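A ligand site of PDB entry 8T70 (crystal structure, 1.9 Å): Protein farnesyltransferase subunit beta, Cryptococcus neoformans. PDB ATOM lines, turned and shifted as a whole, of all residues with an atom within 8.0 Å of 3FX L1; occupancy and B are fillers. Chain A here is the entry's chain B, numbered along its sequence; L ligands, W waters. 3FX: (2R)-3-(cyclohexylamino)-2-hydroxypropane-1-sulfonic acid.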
ATOM      1  N   LEU A  50     -34.267 -20.878   1.322  1.00  0.00           N
ATOM      2  CA  LEU A  50     -33.920 -19.478   1.051  1.00  0.00           C
ATOM      3  C   LEU A  50     -33.022 -18.891   2.136  1.00  0.00           C
ATOM      4  O   LEU A  50     -32.111 -18.101   1.839  1.00  0.00           O
ATOM      5  CB  LEU A  50     -35.197 -18.650   0.893  1.00  0.00           C
ATOM      6  CG  LEU A  50     -35.186 -17.460  -0.066  1.00  0.00           C
ATOM      7  CD1 LEU A  50     -34.358 -16.291   0.465  1.00  0.00           C
ATOM      8  CD2 LEU A  50     -34.687 -17.875  -1.445  1.00  0.00           C
ATOM      9  N   TYR A  58     -24.508 -26.442   7.012  1.00  0.00           N
ATOM     10  CA  TYR A  58     -24.606 -25.733   5.748  1.00  0.00           C
ATOM     11  C   TYR A  58     -23.882 -26.518   4.655  1.00  0.00           C
ATOM     12  O   TYR A  58     -22.718 -26.881   4.808  1.00  0.00           O
ATOM     13  CB  TYR A  58     -24.025 -24.315   5.860  1.00  0.00           C
ATOM     14  CG  TYR A  58     -24.134 -23.565   4.555  1.00  0.00           C
ATOM     15  CD1 TYR A  58     -25.362 -23.405   3.940  1.00  0.00           C
ATOM     16  CD2 TYR A  58     -23.004 -23.079   3.910  1.00  0.00           C
ATOM     17  CE1 TYR A  58     -25.479 -22.762   2.731  1.00  0.00           C
ATOM     18  CE2 TYR A  58     -23.111 -22.433   2.692  1.00  0.00           C
ATOM     19  CZ  TYR A  58     -24.349 -22.280   2.106  1.00  0.00           C
ATOM     20  OH  TYR A  58     -24.476 -21.637   0.898  1.00  0.00           O
ATOM     21  N   GLY A  60     -23.092 -25.650   1.502  1.00  0.00           N
ATOM     22  CA  GLY A  60     -22.347 -24.952   0.462  1.00  0.00           C
ATOM     23  C   GLY A  60     -21.037 -25.614   0.083  1.00  0.00           C
ATOM     24  O   GLY A  60     -20.354 -26.198   0.939  1.00  0.00           O
ATOM     25  N   LEU A  61     -20.681 -25.540  -1.191  1.00  0.00           N
ATOM     26  CA  LEU A  61     -19.461 -26.178  -1.666  1.00  0.00           C
ATOM     27  C   LEU A  61     -18.259 -25.509  -1.027  1.00  0.00           C
ATOM     28  O   LEU A  61     -18.029 -24.306  -1.213  1.00  0.00           O
ATOM     29  CB  LEU A  61     -19.388 -26.106  -3.185  1.00  0.00           C
ATOM     30  CG  LEU A  61     -18.209 -26.873  -3.804  1.00  0.00           C
ATOM     31  CD1 LEU A  61     -18.336 -28.400  -3.599  1.00  0.00           C
ATOM     32  CD2 LEU A  61     -18.156 -26.553  -5.282  1.00  0.00           C
ATOM     33  N   ILE A 486     -27.889 -24.365 -10.665  1.00  0.00           N
ATOM     34  CA  ILE A 486     -26.898 -24.360  -9.604  1.00  0.00           C
ATOM     35  C   ILE A 486     -27.603 -24.504  -8.260  1.00  0.00           C
ATOM     36  O   ILE A 486     -28.023 -23.514  -7.655  1.00  0.00           O
ATOM     37  CB  ILE A 486     -26.027 -23.085  -9.614  1.00  0.00           C
ATOM     38  CG1 ILE A 486     -25.524 -22.767 -11.035  1.00  0.00           C
ATOM     39  CG2 ILE A 486     -24.845 -23.253  -8.639  1.00  0.00           C
ATOM     40  CD1 ILE A 486     -24.693 -23.917 -11.695  1.00  0.00           C
ATOM     41  N   VAL A 487     -27.729 -25.753  -7.809  1.00  0.00           N
ATOM     42  CA  VAL A 487     -28.354 -26.030  -6.510  1.00  0.00           C
ATOM     43  C   VAL A 487     -27.577 -25.313  -5.411  1.00  0.00           C
ATOM     44  O   VAL A 487     -26.346 -25.397  -5.344  1.00  0.00           O
ATOM     45  CB  VAL A 487     -28.411 -27.537  -6.259  1.00  0.00           C
ATOM     46  CG1 VAL A 487     -28.814 -27.828  -4.822  1.00  0.00           C
ATOM     47  CG2 VAL A 487     -29.366 -28.212  -7.242  1.00  0.00           C
ATOM     48  N   GLY A 488     -28.303 -24.606  -4.544  1.00  0.00           N
ATOM     49  CA  GLY A 488     -27.706 -23.929  -3.412  1.00  0.00           C
ATOM     50  C   GLY A 488     -27.208 -22.521  -3.673  1.00  0.00           C
ATOM     51  O   GLY A 488     -26.663 -21.905  -2.751  1.00  0.00           O
ATOM     52  N   GLY A 489     -27.364 -22.011  -4.883  1.00  0.00           N
ATOM     53  CA  GLY A 489     -26.957 -20.660  -5.209  1.00  0.00           C
ATOM     54  C   GLY A 489     -25.645 -20.616  -5.977  1.00  0.00           C
ATOM     55  O   GLY A 489     -24.879 -21.578  -6.032  1.00  0.00           O
ATOM     56  N   LYS A 490     -25.379 -19.432  -6.539  1.00  0.00           N
ATOM     57  CA  LYS A 490     -24.351 -19.305  -7.561  1.00  0.00           C
ATOM     58  C   LYS A 490     -22.944 -19.497  -7.018  1.00  0.00           C
ATOM     59  O   LYS A 490     -22.050 -19.844  -7.797  1.00  0.00           O
ATOM     60  CB  LYS A 490     -24.478 -17.944  -8.259  1.00  0.00           C
ATOM     61  CG  LYS A 490     -25.678 -17.888  -9.199  1.00  0.00           C
ATOM     62  CD  LYS A 490     -25.735 -16.563  -9.959  1.00  0.00           C
ATOM     63  CE  LYS A 490     -26.936 -16.471 -10.880  1.00  0.00           C
ATOM     64  NZ  LYS A 490     -27.131 -15.067 -11.381  1.00  0.00           N
ATOM     65  N   ASP A 491     -22.731 -19.330  -5.710  1.00  0.00           N
ATOM     66  CA  ASP A 491     -21.403 -19.627  -5.162  1.00  0.00           C
ATOM     67  C   ASP A 491     -21.064 -21.116  -5.220  1.00  0.00           C
ATOM     68  O   ASP A 491     -19.899 -21.470  -5.025  1.00  0.00           O
ATOM     69  CB  ASP A 491     -21.311 -19.145  -3.712  1.00  0.00           C
ATOM     70  CG  ASP A 491     -21.191 -17.614  -3.607  1.00  0.00           C
ATOM     71  OD1 ASP A 491     -20.464 -17.004  -4.422  1.00  0.00           O
ATOM     72  OD2 ASP A 491     -21.825 -17.052  -2.695  1.00  0.00           O
ATOM     73  N   ASN A 492     -22.040 -21.983  -5.478  1.00  0.00           N
ATOM     74  CA  ASN A 492     -21.713 -23.390  -5.660  1.00  0.00           C
ATOM     75  C   ASN A 492     -21.285 -23.720  -7.089  1.00  0.00           C
ATOM     76  O   ASN A 492     -20.870 -24.871  -7.342  1.00  0.00           O
ATOM     77  CB  ASN A 492     -22.903 -24.272  -5.290  1.00  0.00           C
ATOM     78  CG  ASN A 492     -23.147 -24.317  -3.803  1.00  0.00           C
ATOM     79  OD1 ASN A 492     -22.240 -24.040  -3.002  1.00  0.00           O
ATOM     80  ND2 ASN A 492     -24.360 -24.668  -3.412  1.00  0.00           N
ATOM     81  N   ARG A 493     -21.382 -22.766  -8.013  1.00  0.00           N
ATOM     82  CA  ARG A 493     -21.124 -23.061  -9.421  1.00  0.00           C
ATOM     83  C   ARG A 493     -19.654 -23.417  -9.621  1.00  0.00           C
ATOM     84  O   ARG A 493     -18.763 -22.725  -9.118  1.00  0.00           O
ATOM     85  CB  ARG A 493     -21.492 -21.865 -10.291  1.00  0.00           C
ATOM     86  CG  ARG A 493     -21.186 -22.079 -11.772  1.00  0.00           C
ATOM     87  CD  ARG A 493     -20.853 -20.771 -12.499  1.00  0.00           C
ATOM     88  NE  ARG A 493     -20.646 -21.010 -13.923  1.00  0.00           N
ATOM     89  CZ  ARG A 493     -19.470 -21.220 -14.505  1.00  0.00           C
ATOM     90  NH1 ARG A 493     -18.343 -21.193 -13.811  1.00  0.00           N
ATOM     91  NH2 ARG A 493     -19.423 -21.468 -15.816  1.00  0.00           N
HETATM   92  OAA 3FX L   1     -28.380 -15.410  -5.852  1.00  0.00           O
HETATM   93  OAB 3FX L   1     -27.318 -17.489  -6.057  1.00  0.00           O
HETATM   94  OAC 3FX L   1     -24.461 -17.168  -4.290  1.00  0.00           O
HETATM   95  OAD 3FX L   1     -25.986 -15.451  -6.469  1.00  0.00           O
HETATM   96  CAE 3FX L   1     -22.055 -16.992   2.149  1.00  0.00           C
HETATM   97  CAF 3FX L   1     -23.254 -16.100   1.821  1.00  0.00           C
HETATM   98  CAG 3FX L   1     -22.349 -18.446   1.736  1.00  0.00           C
HETATM   99  CAH 3FX L   1     -23.610 -16.142   0.340  1.00  0.00           C
HETATM  100  CAI 3FX L   1     -22.744 -18.561   0.258  1.00  0.00           C
HETATM  101  CAJ 3FX L   1     -25.268 -17.033  -1.967  1.00  0.00           C
HETATM  102  CAK 3FX L   1     -26.714 -16.160  -3.824  1.00  0.00           C
HETATM  103  NAL 3FX L   1     -23.960 -17.563  -1.601  1.00  0.00           N
HETATM  104  CAM 3FX L   1     -25.267 -16.442  -3.376  1.00  0.00           C
HETATM  105  CAN 3FX L   1     -23.865 -17.588  -0.144  1.00  0.00           C
HETATM  106  SAO 3FX L   1     -27.053 -16.076  -5.603  1.00  0.00           S
HETATM  107  OAA 3FX L   2     -15.663 -23.648   3.595  1.00  0.00           O
HETATM  108  OAB 3FX L   2     -14.103 -23.669   1.611  1.00  0.00           O
HETATM  109  OAC 3FX L   2     -15.162 -21.449   5.151  1.00  0.00           O
HETATM  110  OAD 3FX L   2     -15.433 -21.797   1.933  1.00  0.00           O
HETATM  111  CAE 3FX L   2     -13.422 -16.229   8.494  1.00  0.00           C
HETATM  112  CAF 3FX L   2     -12.975 -17.406   9.368  1.00  0.00           C
HETATM  113  CAG 3FX L   2     -13.017 -16.397   7.034  1.00  0.00           C
HETATM  114  CAH 3FX L   2     -13.452 -18.735   8.782  1.00  0.00           C
HETATM  115  CAI 3FX L   2     -13.434 -17.745   6.442  1.00  0.00           C
HETATM  116  CAJ 3FX L   2     -12.981 -20.664   5.673  1.00  0.00           C
HETATM  117  CAK 3FX L   2     -13.351 -22.192   3.747  1.00  0.00           C
HETATM  118  NAL 3FX L   2     -13.693 -20.105   6.801  1.00  0.00           N
HETATM  119  CAM 3FX L   2     -13.819 -21.826   5.154  1.00  0.00           C
HETATM  120  CAN 3FX L   2     -13.026 -18.922   7.317  1.00  0.00           C
HETATM  121  SAO 3FX L   2     -14.717 -22.860   2.729  1.00  0.00           S
HETATM  122  O   HOH W   1     -24.343 -20.237  -2.701  1.00  0.00           O
HETATM  123  O   HOH W   2     -29.773 -13.603  -3.917  1.00  0.00           O
HETATM  124  O   HOH W   3     -27.650 -18.898  -1.479  1.00  0.00           O
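A nitrogen (NAL) of 3FX L1 is in salt-bridge range of the side-chain carboxylate (OD2) of Asp 491 (2.5 Å). N of Asp 491 is in hydrogen-bond range of OAC of 3FX L1 (3.1 Å). An oxygen (OAB) of 3FX L1 sits at hydrogen-bond distance from the backbone NH (N) of Lys 490 (2.8 Å).
Tyr 58 touches 3FX L1. Gly 489 touches 3FX L1 (CA to OAB, 3.3 Å).
Water W1 lies within hydrogen-bond range of O of Gly 488 and NAL of 3FX L1.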
